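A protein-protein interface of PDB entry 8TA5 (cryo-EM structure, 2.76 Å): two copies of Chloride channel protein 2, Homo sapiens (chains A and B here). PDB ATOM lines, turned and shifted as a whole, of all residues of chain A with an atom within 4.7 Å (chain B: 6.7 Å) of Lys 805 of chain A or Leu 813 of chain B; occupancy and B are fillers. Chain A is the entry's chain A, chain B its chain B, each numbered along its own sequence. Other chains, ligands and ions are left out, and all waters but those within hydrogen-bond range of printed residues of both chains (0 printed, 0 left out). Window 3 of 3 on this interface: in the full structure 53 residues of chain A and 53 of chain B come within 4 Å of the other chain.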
ATOM      1  N   THR A 801     -12.750 -16.172  14.236  1.00  0.00           N
ATOM      2  CA  THR A 801     -11.923 -16.192  15.434  1.00  0.00           C
ATOM      3  C   THR A 801     -10.865 -15.098  15.363  1.00  0.00           C
ATOM      4  O   THR A 801     -10.228 -14.894  14.326  1.00  0.00           O
ATOM      5  CB  THR A 801     -11.256 -17.556  15.600  1.00  0.00           C
ATOM      6  OG1 THR A 801     -12.208 -18.590  15.329  1.00  0.00           O
ATOM      7  CG2 THR A 801     -10.734 -17.722  17.017  1.00  0.00           C
ATOM      8  N   SER A 802     -10.677 -14.394  16.474  1.00  0.00           N
ATOM      9  CA  SER A 802      -9.717 -13.304  16.515  1.00  0.00           C
ATOM     10  C   SER A 802      -8.295 -13.841  16.652  1.00  0.00           C
ATOM     11  O   SER A 802      -8.067 -14.998  17.016  1.00  0.00           O
ATOM     12  CB  SER A 802     -10.032 -12.351  17.667  1.00  0.00           C
ATOM     13  OG  SER A 802     -10.544 -13.056  18.785  1.00  0.00           O
ATOM     14  N   LEU A 803      -7.328 -12.973  16.344  1.00  0.00           N
ATOM     15  CA  LEU A 803      -5.924 -13.351  16.476  1.00  0.00           C
ATOM     16  C   LEU A 803      -5.549 -13.580  17.935  1.00  0.00           C
ATOM     17  O   LEU A 803      -4.688 -14.414  18.239  1.00  0.00           O
ATOM     18  CB  LEU A 803      -5.032 -12.275  15.855  1.00  0.00           C
ATOM     19  CG  LEU A 803      -3.544 -12.605  15.737  1.00  0.00           C
ATOM     20  CD1 LEU A 803      -3.312 -13.655  14.667  1.00  0.00           C
ATOM     21  CD2 LEU A 803      -2.737 -11.353  15.442  1.00  0.00           C
ATOM     22  N   HIS A 804      -6.181 -12.844  18.851  1.00  0.00           N
ATOM     23  CA  HIS A 804      -5.871 -12.982  20.270  1.00  0.00           C
ATOM     24  C   HIS A 804      -6.166 -14.393  20.767  1.00  0.00           C
ATOM     25  O   HIS A 804      -5.325 -15.023  21.419  1.00  0.00           O
ATOM     26  CB  HIS A 804      -6.662 -11.950  21.074  1.00  0.00           C
ATOM     27  CG  HIS A 804      -6.222 -11.826  22.500  1.00  0.00           C
ATOM     28  ND1 HIS A 804      -5.212 -10.977  22.897  1.00  0.00           N
ATOM     29  CD2 HIS A 804      -6.661 -12.441  23.623  1.00  0.00           C
ATOM     30  CE1 HIS A 804      -5.045 -11.077  24.203  1.00  0.00           C
ATOM     31  NE2 HIS A 804      -5.912 -11.958  24.668  1.00  0.00           N
ATOM     32  N   LYS A 805      -7.362 -14.905  20.464  1.00  0.00           N
ATOM     33  CA  LYS A 805      -7.733 -16.237  20.930  1.00  0.00           C
ATOM     34  C   LYS A 805      -6.862 -17.310  20.291  1.00  0.00           C
ATOM     35  O   LYS A 805      -6.437 -18.255  20.966  1.00  0.00           O
ATOM     36  CB  LYS A 805      -9.210 -16.502  20.643  1.00  0.00           C
ATOM     37  CG  LYS A 805      -9.921 -17.275  21.740  1.00  0.00           C
ATOM     38  CD  LYS A 805     -11.431 -17.176  21.600  1.00  0.00           C
ATOM     39  CE  LYS A 805     -11.965 -18.215  20.627  1.00  0.00           C
ATOM     40  NZ  LYS A 805     -13.155 -17.721  19.879  1.00  0.00           N
ATOM     41  N   THR A 806      -6.591 -17.184  18.990  1.00  0.00           N
ATOM     42  CA  THR A 806      -5.742 -18.158  18.312  1.00  0.00           C
ATOM     43  C   THR A 806      -4.350 -18.186  18.926  1.00  0.00           C
ATOM     44  O   THR A 806      -3.800 -19.258  19.201  1.00  0.00           O
ATOM     45  CB  THR A 806      -5.665 -17.839  16.819  1.00  0.00           C
ATOM     46  OG1 THR A 806      -6.977 -17.546  16.322  1.00  0.00           O
ATOM     47  CG2 THR A 806      -5.087 -19.014  16.052  1.00  0.00           C
ATOM     48  N   HIS A 807      -3.772 -17.006  19.168  1.00  0.00           N
ATOM     49  CA  HIS A 807      -2.453 -16.939  19.786  1.00  0.00           C
ATOM     50  C   HIS A 807      -2.466 -17.536  21.185  1.00  0.00           C
ATOM     51  O   HIS A 807      -1.546 -18.271  21.561  1.00  0.00           O
ATOM     52  CB  HIS A 807      -1.966 -15.490  19.827  1.00  0.00           C
ATOM     53  CG  HIS A 807      -0.542 -15.344  20.261  1.00  0.00           C
ATOM     54  ND1 HIS A 807      -0.174 -15.244  21.586  1.00  0.00           N
ATOM     55  CD2 HIS A 807       0.606 -15.279  19.547  1.00  0.00           C
ATOM     56  CE1 HIS A 807       1.139 -15.125  21.669  1.00  0.00           C
ATOM     57  NE2 HIS A 807       1.636 -15.144  20.445  1.00  0.00           N
ATOM     58  N   THR A 808      -3.502 -17.236  21.972  1.00  0.00           N
ATOM     59  CA  THR A 808      -3.566 -17.743  23.339  1.00  0.00           C
ATOM     60  C   THR A 808      -3.653 -19.267  23.360  1.00  0.00           C
ATOM     61  O   THR A 808      -2.937 -19.933  24.119  1.00  0.00           O
ATOM     62  CB  THR A 808      -4.758 -17.122  24.069  1.00  0.00           C
ATOM     63  OG1 THR A 808      -4.555 -15.711  24.198  1.00  0.00           O
ATOM     64  CG2 THR A 808      -4.911 -17.727  25.450  1.00  0.00           C
ATOM     65  N   ILE A 809      -4.519 -19.839  22.519  1.00  0.00           N
ATOM     66  CA  ILE A 809      -4.675 -21.291  22.506  1.00  0.00           C
ATOM     67  C   ILE A 809      -3.426 -21.964  21.952  1.00  0.00           C
ATOM     68  O   ILE A 809      -3.029 -23.038  22.419  1.00  0.00           O
ATOM     69  CB  ILE A 809      -5.938 -21.699  21.728  1.00  0.00           C
ATOM     70  CG1 ILE A 809      -7.156 -20.942  22.255  1.00  0.00           C
ATOM     71  CG2 ILE A 809      -6.177 -23.187  21.864  1.00  0.00           C
ATOM     72  CD1 ILE A 809      -8.375 -21.061  21.372  1.00  0.00           C
ATOM     73  N   LEU B 171     -14.451 -13.239  36.943  1.00  0.00           N
ATOM     74  CA  LEU B 171     -13.374 -13.482  35.990  1.00  0.00           C
ATOM     75  C   LEU B 171     -13.460 -14.853  35.332  1.00  0.00           C
ATOM     76  O   LEU B 171     -12.729 -15.100  34.367  1.00  0.00           O
ATOM     77  CB  LEU B 171     -12.017 -13.323  36.678  1.00  0.00           C
ATOM     78  CG  LEU B 171     -11.613 -11.897  37.058  1.00  0.00           C
ATOM     79  CD1 LEU B 171     -10.336 -11.901  37.881  1.00  0.00           C
ATOM     80  CD2 LEU B 171     -11.453 -11.036  35.820  1.00  0.00           C
ATOM     81  N   ARG B 172     -14.322 -15.740  35.819  1.00  0.00           N
ATOM     82  CA  ARG B 172     -14.526 -17.051  35.218  1.00  0.00           C
ATOM     83  C   ARG B 172     -15.612 -17.046  34.150  1.00  0.00           C
ATOM     84  O   ARG B 172     -15.950 -18.110  33.623  1.00  0.00           O
ATOM     85  CB  ARG B 172     -14.863 -18.082  36.297  1.00  0.00           C
ATOM     86  CG  ARG B 172     -13.648 -18.711  36.950  1.00  0.00           C
ATOM     87  CD  ARG B 172     -14.045 -19.799  37.934  1.00  0.00           C
ATOM     88  NE  ARG B 172     -14.800 -19.270  39.062  1.00  0.00           N
ATOM     89  CZ  ARG B 172     -14.710 -19.724  40.304  1.00  0.00           C
ATOM     90  NH1 ARG B 172     -13.886 -20.709  40.623  1.00  0.00           N
ATOM     91  NH2 ARG B 172     -15.464 -19.175  41.253  1.00  0.00           N
ATOM     92  N   SER B 234     -12.881  -9.675  25.655  1.00  0.00           N
ATOM     93  CA  SER B 234     -11.548 -10.131  26.036  1.00  0.00           C
ATOM     94  C   SER B 234     -10.728  -9.003  26.649  1.00  0.00           C
ATOM     95  O   SER B 234      -9.868  -9.247  27.503  1.00  0.00           O
ATOM     96  CB  SER B 234     -10.830 -10.715  24.821  1.00  0.00           C
ATOM     97  OG  SER B 234      -9.548 -11.205  25.173  1.00  0.00           O
ATOM     98  N   THR B 237     -11.755  -8.250  30.712  1.00  0.00           N
ATOM     99  CA  THR B 237     -11.324  -9.170  31.763  1.00  0.00           C
ATOM    100  C   THR B 237      -9.876  -8.912  32.171  1.00  0.00           C
ATOM    101  O   THR B 237      -9.536  -8.953  33.363  1.00  0.00           O
ATOM    102  CB  THR B 237     -11.507 -10.613  31.290  1.00  0.00           C
ATOM    103  OG1 THR B 237     -12.892 -10.969  31.374  1.00  0.00           O
ATOM    104  CG2 THR B 237     -10.692 -11.577  32.143  1.00  0.00           C
ATOM    105  N   PHE B 269      -4.628 -19.319  36.213  1.00  0.00           N
ATOM    106  CA  PHE B 269      -3.434 -19.403  35.389  1.00  0.00           C
ATOM    107  C   PHE B 269      -2.539 -18.205  35.666  1.00  0.00           C
ATOM    108  O   PHE B 269      -3.017 -17.110  35.972  1.00  0.00           O
ATOM    109  CB  PHE B 269      -3.780 -19.453  33.895  1.00  0.00           C
ATOM    110  CG  PHE B 269      -4.003 -20.839  33.370  1.00  0.00           C
ATOM    111  CD1 PHE B 269      -2.966 -21.754  33.327  1.00  0.00           C
ATOM    112  CD2 PHE B 269      -5.253 -21.228  32.921  1.00  0.00           C
ATOM    113  CE1 PHE B 269      -3.170 -23.031  32.845  1.00  0.00           C
ATOM    114  CE2 PHE B 269      -5.462 -22.503  32.437  1.00  0.00           C
ATOM    115  CZ  PHE B 269      -4.420 -23.406  32.400  1.00  0.00           C
ATOM    116  N   ALA B 793     -18.685 -15.718  15.894  1.00  0.00           N
ATOM    117  CA  ALA B 793     -17.711 -16.715  16.331  1.00  0.00           C
ATOM    118  C   ALA B 793     -17.799 -16.939  17.834  1.00  0.00           C
ATOM    119  O   ALA B 793     -16.921 -16.499  18.589  1.00  0.00           O
ATOM    120  CB  ALA B 793     -16.293 -16.303  15.936  1.00  0.00           C
ATOM    121  N   PRO B 794     -18.842 -17.615  18.308  1.00  0.00           N
ATOM    122  CA  PRO B 794     -18.772 -18.222  19.640  1.00  0.00           C
ATOM    123  C   PRO B 794     -17.798 -19.387  19.604  1.00  0.00           C
ATOM    124  O   PRO B 794     -17.549 -19.987  18.558  1.00  0.00           O
ATOM    125  CB  PRO B 794     -20.206 -18.694  19.908  1.00  0.00           C
ATOM    126  CG  PRO B 794     -21.046 -18.027  18.856  1.00  0.00           C
ATOM    127  CD  PRO B 794     -20.147 -17.858  17.676  1.00  0.00           C
ATOM    128  N   PHE B 795     -17.234 -19.714  20.759  1.00  0.00           N
ATOM    129  CA  PHE B 795     -16.285 -20.815  20.832  1.00  0.00           C
ATOM    130  C   PHE B 795     -17.057 -22.103  21.085  1.00  0.00           C
ATOM    131  O   PHE B 795     -17.892 -22.170  21.994  1.00  0.00           O
ATOM    132  CB  PHE B 795     -15.212 -20.573  21.901  1.00  0.00           C
ATOM    133  CG  PHE B 795     -15.539 -21.140  23.246  1.00  0.00           C
ATOM    134  CD1 PHE B 795     -16.428 -20.499  24.087  1.00  0.00           C
ATOM    135  CD2 PHE B 795     -14.944 -22.317  23.673  1.00  0.00           C
ATOM    136  CE1 PHE B 795     -16.723 -21.025  25.324  1.00  0.00           C
ATOM    137  CE2 PHE B 795     -15.237 -22.846  24.908  1.00  0.00           C
ATOM    138  CZ  PHE B 795     -16.127 -22.201  25.735  1.00  0.00           C
ATOM    139  N   GLN B 796     -16.818 -23.097  20.243  1.00  0.00           N
ATOM    140  CA  GLN B 796     -17.528 -24.364  20.287  1.00  0.00           C
ATOM    141  C   GLN B 796     -16.564 -25.484  20.657  1.00  0.00           C
ATOM    142  O   GLN B 796     -15.386 -25.261  20.949  1.00  0.00           O
ATOM    143  CB  GLN B 796     -18.205 -24.655  18.945  1.00  0.00           C
ATOM    144  CG  GLN B 796     -19.109 -23.547  18.438  1.00  0.00           C
ATOM    145  CD  GLN B 796     -18.653 -22.998  17.101  1.00  0.00           C
ATOM    146  OE1 GLN B 796     -17.706 -22.221  17.030  1.00  0.00           O
ATOM    147  NE2 GLN B 796     -19.328 -23.404  16.033  1.00  0.00           N
ATOM    148  N   THR B 808      -9.323 -27.755  30.224  1.00  0.00           N
ATOM    149  CA  THR B 808      -8.214 -26.824  30.035  1.00  0.00           C
ATOM    150  C   THR B 808      -8.655 -25.574  29.283  1.00  0.00           C
ATOM    151  O   THR B 808      -8.218 -24.463  29.607  1.00  0.00           O
ATOM    152  CB  THR B 808      -7.067 -27.515  29.298  1.00  0.00           C
ATOM    153  OG1 THR B 808      -6.796 -28.779  29.916  1.00  0.00           O
ATOM    154  CG2 THR B 808      -5.814 -26.661  29.350  1.00  0.00           C
ATOM    155  N   ILE B 809      -9.511 -25.730  28.272  1.00  0.00           N
ATOM    156  CA  ILE B 809      -9.966 -24.576  27.501  1.00  0.00           C
ATOM    157  C   ILE B 809     -10.866 -23.685  28.349  1.00  0.00           C
ATOM    158  O   ILE B 809     -10.819 -22.453  28.244  1.00  0.00           O
ATOM    159  CB  ILE B 809     -10.668 -25.040  26.212  1.00  0.00           C
ATOM    160  CG1 ILE B 809      -9.697 -25.830  25.333  1.00  0.00           C
ATOM    161  CG2 ILE B 809     -11.216 -23.852  25.440  1.00  0.00           C
ATOM    162  CD1 ILE B 809      -8.598 -24.989  24.731  1.00  0.00           C
ATOM    163  N   PHE B 810     -11.701 -24.288  29.200  1.00  0.00           N
ATOM    164  CA  PHE B 810     -12.590 -23.504  30.051  1.00  0.00           C
ATOM    165  C   PHE B 810     -11.805 -22.626  31.018  1.00  0.00           C
ATOM    166  O   PHE B 810     -12.151 -21.459  31.230  1.00  0.00           O
ATOM    167  CB  PHE B 810     -13.532 -24.431  30.818  1.00  0.00           C
ATOM    168  CG  PHE B 810     -14.904 -24.530  30.219  1.00  0.00           C
ATOM    169  CD1 PHE B 810     -15.140 -25.348  29.128  1.00  0.00           C
ATOM    170  CD2 PHE B 810     -15.957 -23.805  30.747  1.00  0.00           C
ATOM    171  CE1 PHE B 810     -16.400 -25.440  28.576  1.00  0.00           C
ATOM    172  CE2 PHE B 810     -17.220 -23.893  30.198  1.00  0.00           C
ATOM    173  CZ  PHE B 810     -17.441 -24.712  29.111  1.00  0.00           C
ATOM    174  N   SER B 811     -10.747 -23.176  31.620  1.00  0.00           N
ATOM    175  CA  SER B 811      -9.939 -22.398  32.555  1.00  0.00           C
ATOM    176  C   SER B 811      -9.190 -21.278  31.844  1.00  0.00           C
ATOM    177  O   SER B 811      -9.060 -20.172  32.380  1.00  0.00           O
ATOM    178  CB  SER B 811      -8.961 -23.315  33.288  1.00  0.00           C
ATOM    179  OG  SER B 811      -9.598 -24.512  33.699  1.00  0.00           O
ATOM    180  N   LEU B 812      -8.686 -21.549  30.639  1.00  0.00           N
ATOM    181  CA  LEU B 812      -7.880 -20.563  29.926  1.00  0.00           C
ATOM    182  C   LEU B 812      -8.715 -19.370  29.477  1.00  0.00           C
ATOM    183  O   LEU B 812      -8.336 -18.215  29.700  1.00  0.00           O
ATOM    184  CB  LEU B 812      -7.210 -21.217  28.721  1.00  0.00           C
ATOM    185  CG  LEU B 812      -6.383 -20.275  27.846  1.00  0.00           C
ATOM    186  CD1 LEU B 812      -5.314 -19.571  28.667  1.00  0.00           C
ATOM    187  CD2 LEU B 812      -5.782 -21.018  26.670  1.00  0.00           C
ATOM    188  N   LEU B 813      -9.856 -19.630  28.842  1.00  0.00           N
ATOM    189  CA  LEU B 813     -10.579 -18.590  28.124  1.00  0.00           C
ATOM    190  C   LEU B 813     -11.454 -17.725  29.022  1.00  0.00           C
ATOM    191  O   LEU B 813     -11.958 -16.699  28.555  1.00  0.00           O
ATOM    192  CB  LEU B 813     -11.437 -19.219  27.024  1.00  0.00           C
ATOM    193  CG  LEU B 813     -10.671 -19.740  25.805  1.00  0.00           C
ATOM    194  CD1 LEU B 813     -11.630 -20.128  24.692  1.00  0.00           C
ATOM    195  CD2 LEU B 813      -9.668 -18.705  25.318  1.00  0.00           C
ATOM    196  N   GLY B 814     -11.642 -18.100  30.285  1.00  0.00           N
ATOM    197  CA  GLY B 814     -12.488 -17.325  31.170  1.00  0.00           C
ATOM    198  C   GLY B 814     -13.936 -17.305  30.722  1.00  0.00           C
ATOM    199  O   GLY B 814     -14.571 -16.247  30.690  1.00  0.00           O
ATOM    200  N   VAL B 815     -14.463 -18.475  30.369  1.00  0.00           N
ATOM    201  CA  VAL B 815     -15.819 -18.611  29.861  1.00  0.00           C
ATOM    202  C   VAL B 815     -16.580 -19.587  30.748  1.00  0.00           C
ATOM    203  O   VAL B 815     -16.000 -20.298  31.572  1.00  0.00           O
ATOM    204  CB  VAL B 815     -15.837 -19.082  28.395  1.00  0.00           C
ATOM    205  CG1 VAL B 815     -15.493 -17.931  27.466  1.00  0.00           C
ATOM    206  CG2 VAL B 815     -14.853 -20.217  28.212  1.00  0.00           C
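Printed residues of chain B that touch a printed residue of chain A: Ser 234, Ala 793, Leu 812 and Leu 813. Of the 9 printed residues of chain A, 4 touch a printed residue of chain B. Hydrophobic or aromatic side chains of chain A that line the printed part of chain B: His 804. Among the printed residues, 4 pairs touch across the chains.
2 positions are printed for both chains. Of the 4 pairs that touch across the chains among the printed residues, none has its exchanged pair printed and touching as well.
N of Thr 801 of chain A touches CB of Ala 793 of chain B, at 3.9 Å. OG of Ser 234 of chain B touches CD2 of His 804 of chain A, at 3.5 Å. CG of Lys 805 of chain A touches CD2 of Leu 813 of chain B (3.9 Å). Thr 808 of chain A touches Leu 812 of chain B (CG2 to CD2, 3.6 Å).
O of His 804 of chain A is in hydrogen-bond range of OG1 of Thr 808 of chain A, 3.0 Å away.
Of the printed residues of chain B, Thr 801 of chain A touches Ala 793. Of the printed residues of chain B, His 804 of chain A touches Ser 234. Printed residues of chain B within 4 Å of Thr 808 of chain A: Leu 812. Of the printed residues of chain A, Ser 234 of chain B touches His 804 (3.5 Å). The nearest residue of chain B that does not touch Lys 805 of chain A is Phe 795 of chain B (4.1 Å). The nearest residue of chain A that does not touch Leu 813 of chain B is Ile 809 of chain A (4.5 Å).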
